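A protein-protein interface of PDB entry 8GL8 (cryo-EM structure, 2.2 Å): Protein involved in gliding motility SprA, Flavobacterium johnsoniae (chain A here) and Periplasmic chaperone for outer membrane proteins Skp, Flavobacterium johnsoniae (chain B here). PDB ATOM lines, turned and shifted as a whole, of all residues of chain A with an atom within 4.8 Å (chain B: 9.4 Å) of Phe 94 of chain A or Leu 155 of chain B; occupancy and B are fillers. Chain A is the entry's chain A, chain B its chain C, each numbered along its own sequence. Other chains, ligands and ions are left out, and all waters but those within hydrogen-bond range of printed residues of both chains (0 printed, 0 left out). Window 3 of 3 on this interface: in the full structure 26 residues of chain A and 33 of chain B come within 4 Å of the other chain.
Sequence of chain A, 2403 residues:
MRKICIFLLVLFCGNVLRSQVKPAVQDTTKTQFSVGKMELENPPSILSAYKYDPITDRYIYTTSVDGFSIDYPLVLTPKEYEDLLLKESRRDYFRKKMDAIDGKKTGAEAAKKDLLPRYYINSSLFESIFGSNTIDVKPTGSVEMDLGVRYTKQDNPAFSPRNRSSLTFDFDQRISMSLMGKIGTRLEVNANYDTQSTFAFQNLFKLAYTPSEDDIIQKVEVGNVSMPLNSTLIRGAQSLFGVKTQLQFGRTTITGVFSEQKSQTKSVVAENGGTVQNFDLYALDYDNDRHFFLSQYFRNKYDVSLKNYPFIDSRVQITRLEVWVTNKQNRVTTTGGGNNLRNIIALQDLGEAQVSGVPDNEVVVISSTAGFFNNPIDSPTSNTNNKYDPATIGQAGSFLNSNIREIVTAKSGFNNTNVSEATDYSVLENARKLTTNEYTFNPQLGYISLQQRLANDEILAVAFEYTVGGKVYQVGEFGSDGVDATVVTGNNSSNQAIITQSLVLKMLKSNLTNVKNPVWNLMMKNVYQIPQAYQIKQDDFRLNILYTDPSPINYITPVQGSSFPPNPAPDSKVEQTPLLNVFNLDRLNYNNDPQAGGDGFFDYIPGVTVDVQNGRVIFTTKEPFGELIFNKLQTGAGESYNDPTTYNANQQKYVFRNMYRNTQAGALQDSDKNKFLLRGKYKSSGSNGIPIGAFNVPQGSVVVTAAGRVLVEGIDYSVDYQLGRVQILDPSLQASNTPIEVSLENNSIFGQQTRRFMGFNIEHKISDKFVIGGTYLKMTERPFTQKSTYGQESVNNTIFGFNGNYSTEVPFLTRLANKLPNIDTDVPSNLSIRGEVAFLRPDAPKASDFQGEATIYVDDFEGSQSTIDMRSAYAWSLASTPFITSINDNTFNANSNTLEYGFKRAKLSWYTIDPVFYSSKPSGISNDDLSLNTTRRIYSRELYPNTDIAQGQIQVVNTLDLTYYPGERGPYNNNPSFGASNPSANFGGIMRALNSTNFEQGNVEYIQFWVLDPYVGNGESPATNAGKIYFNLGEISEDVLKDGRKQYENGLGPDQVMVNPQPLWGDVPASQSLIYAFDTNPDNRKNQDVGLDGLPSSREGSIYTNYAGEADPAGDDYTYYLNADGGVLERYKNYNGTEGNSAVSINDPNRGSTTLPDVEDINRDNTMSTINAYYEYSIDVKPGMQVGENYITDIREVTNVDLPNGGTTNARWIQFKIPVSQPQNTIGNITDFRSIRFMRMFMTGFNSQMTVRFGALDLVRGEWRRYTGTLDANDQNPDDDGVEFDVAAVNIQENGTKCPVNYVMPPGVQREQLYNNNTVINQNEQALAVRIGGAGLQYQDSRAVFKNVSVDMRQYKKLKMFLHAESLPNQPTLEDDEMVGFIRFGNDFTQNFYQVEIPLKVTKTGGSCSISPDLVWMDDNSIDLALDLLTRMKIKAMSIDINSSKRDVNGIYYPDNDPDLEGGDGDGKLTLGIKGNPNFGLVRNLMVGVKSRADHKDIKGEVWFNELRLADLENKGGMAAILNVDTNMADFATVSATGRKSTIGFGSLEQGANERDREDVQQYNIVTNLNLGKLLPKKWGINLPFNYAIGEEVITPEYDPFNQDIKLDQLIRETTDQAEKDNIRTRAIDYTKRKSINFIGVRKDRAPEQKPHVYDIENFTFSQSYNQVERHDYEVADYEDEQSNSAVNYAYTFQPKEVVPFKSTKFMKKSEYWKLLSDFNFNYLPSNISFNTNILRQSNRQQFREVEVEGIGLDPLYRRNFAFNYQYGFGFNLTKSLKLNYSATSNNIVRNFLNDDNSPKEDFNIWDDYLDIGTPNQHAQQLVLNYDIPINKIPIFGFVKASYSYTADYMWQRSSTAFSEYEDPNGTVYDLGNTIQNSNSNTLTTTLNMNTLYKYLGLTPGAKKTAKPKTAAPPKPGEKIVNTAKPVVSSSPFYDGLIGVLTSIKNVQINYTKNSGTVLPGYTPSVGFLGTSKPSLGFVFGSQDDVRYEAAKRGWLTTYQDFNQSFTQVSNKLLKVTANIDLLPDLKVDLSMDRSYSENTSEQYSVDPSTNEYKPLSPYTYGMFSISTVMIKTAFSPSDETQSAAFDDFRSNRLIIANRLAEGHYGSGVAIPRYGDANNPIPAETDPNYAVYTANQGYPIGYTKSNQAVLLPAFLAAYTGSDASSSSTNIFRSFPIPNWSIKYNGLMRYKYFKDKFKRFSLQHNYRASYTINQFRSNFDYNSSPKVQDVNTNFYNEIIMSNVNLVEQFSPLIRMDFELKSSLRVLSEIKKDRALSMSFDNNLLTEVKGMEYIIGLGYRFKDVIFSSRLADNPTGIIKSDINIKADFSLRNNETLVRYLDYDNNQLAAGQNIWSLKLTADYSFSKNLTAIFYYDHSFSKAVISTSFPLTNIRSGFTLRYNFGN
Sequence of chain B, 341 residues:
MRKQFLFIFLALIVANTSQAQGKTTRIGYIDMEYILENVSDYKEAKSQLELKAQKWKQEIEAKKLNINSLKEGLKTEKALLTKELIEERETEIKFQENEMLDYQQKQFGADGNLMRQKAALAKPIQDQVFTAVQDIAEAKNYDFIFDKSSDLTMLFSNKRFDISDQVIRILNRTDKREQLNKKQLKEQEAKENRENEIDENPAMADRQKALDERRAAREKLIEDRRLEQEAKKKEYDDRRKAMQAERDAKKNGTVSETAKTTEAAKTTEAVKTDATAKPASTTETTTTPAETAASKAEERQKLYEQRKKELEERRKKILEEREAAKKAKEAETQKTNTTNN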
ATOM      1  N   ARG A  90     -12.281   6.539   8.510  1.00  0.00           N
ATOM      2  CA  ARG A  90     -12.769   6.184   9.839  1.00  0.00           C
ATOM      3  C   ARG A  90     -12.327   4.779  10.223  1.00  0.00           C
ATOM      4  O   ARG A  90     -11.866   4.540  11.348  1.00  0.00           O
ATOM      5  CB  ARG A  90     -14.292   6.295   9.883  1.00  0.00           C
ATOM      6  CG  ARG A  90     -14.821   7.715   9.865  1.00  0.00           C
ATOM      7  CD  ARG A  90     -16.232   7.779  10.414  1.00  0.00           C
ATOM      8  NE  ARG A  90     -17.176   7.064   9.565  1.00  0.00           N
ATOM      9  CZ  ARG A  90     -17.761   7.583   8.494  1.00  0.00           C
ATOM     10  NH1 ARG A  90     -17.527   8.828   8.115  1.00  0.00           N
ATOM     11  NH2 ARG A  90     -18.602   6.835   7.788  1.00  0.00           N
ATOM     12  N   ARG A  91     -12.455   3.833   9.288  1.00  0.00           N
ATOM     13  CA  ARG A  91     -12.036   2.464   9.570  1.00  0.00           C
ATOM     14  C   ARG A  91     -10.541   2.395   9.856  1.00  0.00           C
ATOM     15  O   ARG A  91     -10.112   1.709  10.790  1.00  0.00           O
ATOM     16  CB  ARG A  91     -12.408   1.555   8.399  1.00  0.00           C
ATOM     17  CG  ARG A  91     -11.624   0.259   8.335  1.00  0.00           C
ATOM     18  CD  ARG A  91     -11.974  -0.533   7.090  1.00  0.00           C
ATOM     19  NE  ARG A  91     -13.393  -0.448   6.766  1.00  0.00           N
ATOM     20  CZ  ARG A  91     -13.871  -0.074   5.587  1.00  0.00           C
ATOM     21  NH1 ARG A  91     -13.069   0.265   4.593  1.00  0.00           N
ATOM     22  NH2 ARG A  91     -15.186  -0.041   5.402  1.00  0.00           N
ATOM     23  N   ASP A  92      -9.734   3.113   9.072  1.00  0.00           N
ATOM     24  CA  ASP A  92      -8.290   3.107   9.275  1.00  0.00           C
ATOM     25  C   ASP A  92      -7.910   3.760  10.598  1.00  0.00           C
ATOM     26  O   ASP A  92      -6.993   3.295  11.280  1.00  0.00           O
ATOM     27  CB  ASP A  92      -7.597   3.812   8.111  1.00  0.00           C
ATOM     28  CG  ASP A  92      -7.199   2.856   7.008  1.00  0.00           C
ATOM     29  OD1 ASP A  92      -7.175   1.634   7.261  1.00  0.00           O
ATOM     30  OD2 ASP A  92      -6.914   3.325   5.887  1.00  0.00           O
ATOM     31  N   TYR A  93      -8.595   4.843  10.970  1.00  0.00           N
ATOM     32  CA  TYR A  93      -8.323   5.495  12.246  1.00  0.00           C
ATOM     33  C   TYR A  93      -8.613   4.558  13.410  1.00  0.00           C
ATOM     34  O   TYR A  93      -7.792   4.407  14.324  1.00  0.00           O
ATOM     35  CB  TYR A  93      -9.156   6.771  12.357  1.00  0.00           C
ATOM     36  CG  TYR A  93      -8.789   7.660  13.520  1.00  0.00           C
ATOM     37  CD1 TYR A  93      -7.621   8.407  13.504  1.00  0.00           C
ATOM     38  CD2 TYR A  93      -9.615   7.759  14.628  1.00  0.00           C
ATOM     39  CE1 TYR A  93      -7.285   9.222  14.563  1.00  0.00           C
ATOM     40  CE2 TYR A  93      -9.288   8.571  15.688  1.00  0.00           C
ATOM     41  CZ  TYR A  93      -8.122   9.301  15.652  1.00  0.00           C
ATOM     42  OH  TYR A  93      -7.791  10.114  16.709  1.00  0.00           O
ATOM     43  N   PHE A  94      -9.776   3.900  13.382  1.00  0.00           N
ATOM     44  CA  PHE A  94     -10.097   2.949  14.439  1.00  0.00           C
ATOM     45  C   PHE A  94      -9.088   1.808  14.477  1.00  0.00           C
ATOM     46  O   PHE A  94      -8.616   1.419  15.554  1.00  0.00           O
ATOM     47  CB  PHE A  94     -11.512   2.405  14.247  1.00  0.00           C
ATOM     48  CG  PHE A  94     -12.587   3.313  14.767  1.00  0.00           C
ATOM     49  CD1 PHE A  94     -12.417   4.004  15.953  1.00  0.00           C
ATOM     50  CD2 PHE A  94     -13.774   3.471  14.072  1.00  0.00           C
ATOM     51  CE1 PHE A  94     -13.405   4.837  16.432  1.00  0.00           C
ATOM     52  CE2 PHE A  94     -14.765   4.302  14.547  1.00  0.00           C
ATOM     53  CZ  PHE A  94     -14.581   4.986  15.729  1.00  0.00           C
ATOM     54  N   ARG A  95      -8.736   1.267  13.308  1.00  0.00           N
ATOM     55  CA  ARG A  95      -7.809   0.144  13.257  1.00  0.00           C
ATOM     56  C   ARG A  95      -6.442   0.532  13.803  1.00  0.00           C
ATOM     57  O   ARG A  95      -5.836  -0.226  14.564  1.00  0.00           O
ATOM     58  CB  ARG A  95      -7.688  -0.369  11.823  1.00  0.00           C
ATOM     59  CG  ARG A  95      -6.623  -1.429  11.628  1.00  0.00           C
ATOM     60  CD  ARG A  95      -7.127  -2.558  10.749  1.00  0.00           C
ATOM     61  NE  ARG A  95      -8.563  -2.765  10.903  1.00  0.00           N
ATOM     62  CZ  ARG A  95      -9.421  -2.823   9.895  1.00  0.00           C
ATOM     63  NH1 ARG A  95      -9.025  -2.685   8.641  1.00  0.00           N
ATOM     64  NH2 ARG A  95     -10.711  -3.022  10.152  1.00  0.00           N
ATOM     65  N   LYS A  96      -5.945   1.713  13.432  1.00  0.00           N
ATOM     66  CA  LYS A  96      -4.655   2.168  13.937  1.00  0.00           C
ATOM     67  C   LYS A  96      -4.700   2.390  15.442  1.00  0.00           C
ATOM     68  O   LYS A  96      -3.738   2.071  16.151  1.00  0.00           O
ATOM     69  CB  LYS A  96      -4.231   3.447  13.216  1.00  0.00           C
ATOM     70  CG  LYS A  96      -3.649   3.212  11.833  1.00  0.00           C
ATOM     71  CD  LYS A  96      -3.198   4.515  11.193  1.00  0.00           C
ATOM     72  CE  LYS A  96      -4.250   5.051  10.234  1.00  0.00           C
ATOM     73  NZ  LYS A  96      -4.513   6.501  10.441  1.00  0.00           N
ATOM     74  N   LYS A  97      -5.808   2.931  15.952  1.00  0.00           N
ATOM     75  CA  LYS A  97      -5.913   3.156  17.389  1.00  0.00           C
ATOM     76  C   LYS A  97      -5.863   1.841  18.162  1.00  0.00           C
ATOM     77  O   LYS A  97      -5.118   1.713  19.142  1.00  0.00           O
ATOM     78  CB  LYS A  97      -7.194   3.925  17.708  1.00  0.00           C
ATOM     79  CG  LYS A  97      -7.417   4.159  19.186  1.00  0.00           C
ATOM     80  CD  LYS A  97      -8.761   4.807  19.435  1.00  0.00           C
ATOM     81  CE  LYS A  97      -8.833   6.180  18.794  1.00  0.00           C
ATOM     82  NZ  LYS A  97      -8.440   7.248  19.750  1.00  0.00           N
ATOM     83  N   MET A  98      -6.636   0.841  17.729  1.00  0.00           N
ATOM     84  CA  MET A  98      -6.601  -0.425  18.462  1.00  0.00           C
ATOM     85  C   MET A  98      -5.316  -1.207  18.206  1.00  0.00           C
ATOM     86  O   MET A  98      -4.907  -2.004  19.057  1.00  0.00           O
ATOM     87  CB  MET A  98      -7.822  -1.287  18.150  1.00  0.00           C
ATOM     88  CG  MET A  98      -9.033  -0.520  17.700  1.00  0.00           C
ATOM     89  SD  MET A  98     -10.500  -1.548  17.608  1.00  0.00           S
ATOM     90  CE  MET A  98     -10.513  -2.247  19.256  1.00  0.00           C
ATOM     91  N   TYR B  29     -11.974 -14.152  17.590  1.00  0.00           N
ATOM     92  CA  TYR B  29     -11.422 -13.368  16.496  1.00  0.00           C
ATOM     93  C   TYR B  29      -9.949 -13.706  16.334  1.00  0.00           C
ATOM     94  O   TYR B  29      -9.306 -14.230  17.245  1.00  0.00           O
ATOM     95  CB  TYR B  29     -11.634 -11.863  16.703  1.00  0.00           C
ATOM     96  CG  TYR B  29     -11.077 -11.296  17.985  1.00  0.00           C
ATOM     97  CD1 TYR B  29     -11.756 -11.441  19.185  1.00  0.00           C
ATOM     98  CD2 TYR B  29      -9.887 -10.591  17.989  1.00  0.00           C
ATOM     99  CE1 TYR B  29     -11.255 -10.915  20.352  1.00  0.00           C
ATOM    100  CE2 TYR B  29      -9.380 -10.061  19.148  1.00  0.00           C
ATOM    101  CZ  TYR B  29     -10.067 -10.224  20.327  1.00  0.00           C
ATOM    102  OH  TYR B  29      -9.556  -9.693  21.484  1.00  0.00           O
ATOM    103  N   LYS B 148     -10.301  -9.479  12.958  1.00  0.00           N
ATOM    104  CA  LYS B 148     -10.251  -8.121  13.486  1.00  0.00           C
ATOM    105  C   LYS B 148      -9.648  -7.134  12.499  1.00  0.00           C
ATOM    106  O   LYS B 148      -9.850  -5.926  12.649  1.00  0.00           O
ATOM    107  CB  LYS B 148      -9.457  -8.092  14.791  1.00  0.00           C
ATOM    108  CG  LYS B 148     -10.273  -7.678  15.998  1.00  0.00           C
ATOM    109  CD  LYS B 148      -9.393  -7.103  17.092  1.00  0.00           C
ATOM    110  CE  LYS B 148      -9.862  -5.720  17.506  1.00  0.00           C
ATOM    111  NZ  LYS B 148     -10.049  -5.616  18.980  1.00  0.00           N
ATOM    112  N   SER B 150     -10.280  -7.090   9.198  1.00  0.00           N
ATOM    113  CA  SER B 150     -11.099  -7.034   7.999  1.00  0.00           C
ATOM    114  C   SER B 150     -11.804  -5.680   7.918  1.00  0.00           C
ATOM    115  O   SER B 150     -11.509  -4.754   8.676  1.00  0.00           O
ATOM    116  CB  SER B 150     -12.090  -8.193   7.989  1.00  0.00           C
ATOM    117  OG  SER B 150     -12.757  -8.296   9.233  1.00  0.00           O
ATOM    118  N   ASP B 151     -12.748  -5.554   6.983  1.00  0.00           N
ATOM    119  CA  ASP B 151     -13.456  -4.290   6.812  1.00  0.00           C
ATOM    120  C   ASP B 151     -14.408  -4.013   7.968  1.00  0.00           C
ATOM    121  O   ASP B 151     -14.627  -2.848   8.320  1.00  0.00           O
ATOM    122  CB  ASP B 151     -14.215  -4.288   5.487  1.00  0.00           C
ATOM    123  CG  ASP B 151     -13.367  -3.794   4.333  1.00  0.00           C
ATOM    124  OD1 ASP B 151     -12.147  -3.616   4.525  1.00  0.00           O
ATOM    125  OD2 ASP B 151     -13.922  -3.581   3.234  1.00  0.00           O
ATOM    126  N   LEU B 152     -14.981  -5.053   8.565  1.00  0.00           N
ATOM    127  CA  LEU B 152     -15.849  -4.882   9.722  1.00  0.00           C
ATOM    128  C   LEU B 152     -14.992  -4.619  10.952  1.00  0.00           C
ATOM    129  O   LEU B 152     -14.117  -5.423  11.288  1.00  0.00           O
ATOM    130  CB  LEU B 152     -16.720  -6.117   9.924  1.00  0.00           C
ATOM    131  CG  LEU B 152     -17.633  -6.116  11.150  1.00  0.00           C
ATOM    132  CD1 LEU B 152     -18.627  -4.971  11.074  1.00  0.00           C
ATOM    133  CD2 LEU B 152     -18.354  -7.444  11.280  1.00  0.00           C
ATOM    134  N   THR B 153     -15.242  -3.499  11.622  1.00  0.00           N
ATOM    135  CA  THR B 153     -14.432  -3.070  12.753  1.00  0.00           C
ATOM    136  C   THR B 153     -15.166  -3.349  14.057  1.00  0.00           C
ATOM    137  O   THR B 153     -16.343  -3.006  14.197  1.00  0.00           O
ATOM    138  CB  THR B 153     -14.098  -1.582  12.658  1.00  0.00           C
ATOM    139  OG1 THR B 153     -15.164  -0.815  13.226  1.00  0.00           O
ATOM    140  CG2 THR B 153     -13.905  -1.171  11.211  1.00  0.00           C
ATOM    141  N   MET B 154     -14.470  -3.974  15.001  1.00  0.00           N
ATOM    142  CA  MET B 154     -14.970  -4.145  16.357  1.00  0.00           C
ATOM    143  C   MET B 154     -14.335  -3.079  17.235  1.00  0.00           C
ATOM    144  O   MET B 154     -13.118  -3.089  17.440  1.00  0.00           O
ATOM    145  CB  MET B 154     -14.646  -5.529  16.913  1.00  0.00           C
ATOM    146  CG  MET B 154     -14.435  -6.605  15.884  1.00  0.00           C
ATOM    147  SD  MET B 154     -13.737  -8.073  16.657  1.00  0.00           S
ATOM    148  CE  MET B 154     -13.777  -9.211  15.284  1.00  0.00           C
ATOM    149  N   LEU B 155     -15.152  -2.166  17.757  1.00  0.00           N
ATOM    150  CA  LEU B 155     -14.624  -1.157  18.662  1.00  0.00           C
ATOM    151  C   LEU B 155     -14.281  -1.735  20.024  1.00  0.00           C
ATOM    152  O   LEU B 155     -13.508  -1.125  20.767  1.00  0.00           O
ATOM    153  CB  LEU B 155     -15.622  -0.012  18.813  1.00  0.00           C
ATOM    154  CG  LEU B 155     -15.984   0.725  17.528  1.00  0.00           C
ATOM    155  CD1 LEU B 155     -16.676   2.023  17.859  1.00  0.00           C
ATOM    156  CD2 LEU B 155     -14.741   0.982  16.701  1.00  0.00           C
ATOM    157  N   PHE B 156     -14.834  -2.894  20.366  1.00  0.00           N
ATOM    158  CA  PHE B 156     -14.542  -3.551  21.628  1.00  0.00           C
ATOM    159  C   PHE B 156     -14.443  -5.051  21.405  1.00  0.00           C
ATOM    160  O   PHE B 156     -15.253  -5.635  20.682  1.00  0.00           O
ATOM    161  CB  PHE B 156     -15.613  -3.250  22.680  1.00  0.00           C
ATOM    162  CG  PHE B 156     -15.321  -3.849  24.021  1.00  0.00           C
ATOM    163  CD1 PHE B 156     -14.454  -3.223  24.895  1.00  0.00           C
ATOM    164  CD2 PHE B 156     -15.904  -5.041  24.403  1.00  0.00           C
ATOM    165  CE1 PHE B 156     -14.178  -3.773  26.125  1.00  0.00           C
ATOM    166  CE2 PHE B 156     -15.630  -5.595  25.632  1.00  0.00           C
ATOM    167  CZ  PHE B 156     -14.766  -4.961  26.494  1.00  0.00           C
ATOM    168  N   SER B 157     -13.443  -5.665  22.030  1.00  0.00           N
ATOM    169  CA  SER B 157     -13.271  -7.109  22.017  1.00  0.00           C
ATOM    170  C   SER B 157     -12.900  -7.562  23.420  1.00  0.00           C
ATOM    171  O   SER B 157     -12.136  -6.886  24.114  1.00  0.00           O
ATOM    172  CB  SER B 157     -12.196  -7.538  21.017  1.00  0.00           C
ATOM    173  OG  SER B 157     -12.754  -7.741  19.732  1.00  0.00           O
ATOM    174  N   ASN B 158     -13.436  -8.710  23.831  1.00  0.00           N
ATOM    175  CA  ASN B 158     -13.263  -9.165  25.206  1.00  0.00           C
ATOM    176  C   ASN B 158     -11.838  -9.599  25.520  1.00  0.00           C
ATOM    177  O   ASN B 158     -11.525  -9.808  26.697  1.00  0.00           O
ATOM    178  CB  ASN B 158     -14.230 -10.307  25.502  1.00  0.00           C
ATOM    179  CG  ASN B 158     -14.509 -10.462  26.980  1.00  0.00           C
ATOM    180  OD1 ASN B 158     -14.451  -9.495  27.737  1.00  0.00           O
ATOM    181  ND2 ASN B 158     -14.827 -11.679  27.398  1.00  0.00           N
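NH1 of Arg 91 of chain A is in salt-bridge range of OD1 of Asp 151 of chain B, 3.99 Å away.
The backbone carbonyl oxygen (O) of Met 154 of chain B lies close to the side-chain sulfur (SD) of Met 98 of chain A (3.0 Å).
O of Ser 150 of chain B lies within hydrogen-bond range of NH2 of Arg 95 of chain A.
OG of Ser 157 of chain B sits at hydrogen-bond distance from SD of Met 154 of chain B (3.2 Å).
Among the printed residues, merely in contact across the chains: Arg 91 of chain A with Thr 153 of chain B (3.9 Å), Phe 94 of chain A with Leu 155 of chain B (3.7 Å), Arg 95 of chain A with Lys 148 of chain B (3.8 Å), Arg 95 of chain A with Thr 153 of chain B (3.8 Å), Met 98 of chain A with Lys 148 of chain B (3.4 Å) and Met 98 of chain A with Leu 155 of chain B (3.5 Å).
Arg 90 of chain A touches none of the printed residues of chain B.
Printed residues of chain B within 4 Å of Arg 91 of chain A: Asp 151 and Thr 153.
Printed residues of chain B within 4 Å of Phe 94 of chain A: Leu 155 (3.7 Å).
Of the printed residues of chain B, Arg 95 of chain A touches Lys 148, Ser 150 and Thr 153.
Printed residues of chain A within 4 Å of Lys 148 of chain B: Arg 95 (3.8 Å) and Met 98 (3.4 Å).
Of the printed residues of chain A, Asp 151 of chain B touches Arg 91.
Of the printed residues of chain A, Thr 153 of chain B touches Arg 91 (3.9 Å) and Arg 95 (3.8 Å).
The nearest residue of chain B that does not touch Phe 94 of chain A is Thr 153 of chain B (4.6 Å).
The nearest printed residue of chain A that does not touch Leu 155 of chain B is Arg 95 of chain A (6.9 Å).
Hydrophobic or aromatic side chains of chain B within 4 Å of the printed part of chain A: Leu 155.
Of the 9 printed residues of chain A, 4 touch a printed residue of chain B.
Hydrophobic or aromatic side chains of chain A that line the printed part of chain B: Phe 94 and Met 98.
Among the printed residues, 9 pairs touch across the chains.
Among the printed residues, Asp or Glu carboxylates within 4 Å of a Lys or Arg side-chain nitrogen of the other chain: Arg 91 of chain A with Asp 151 of chain B.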
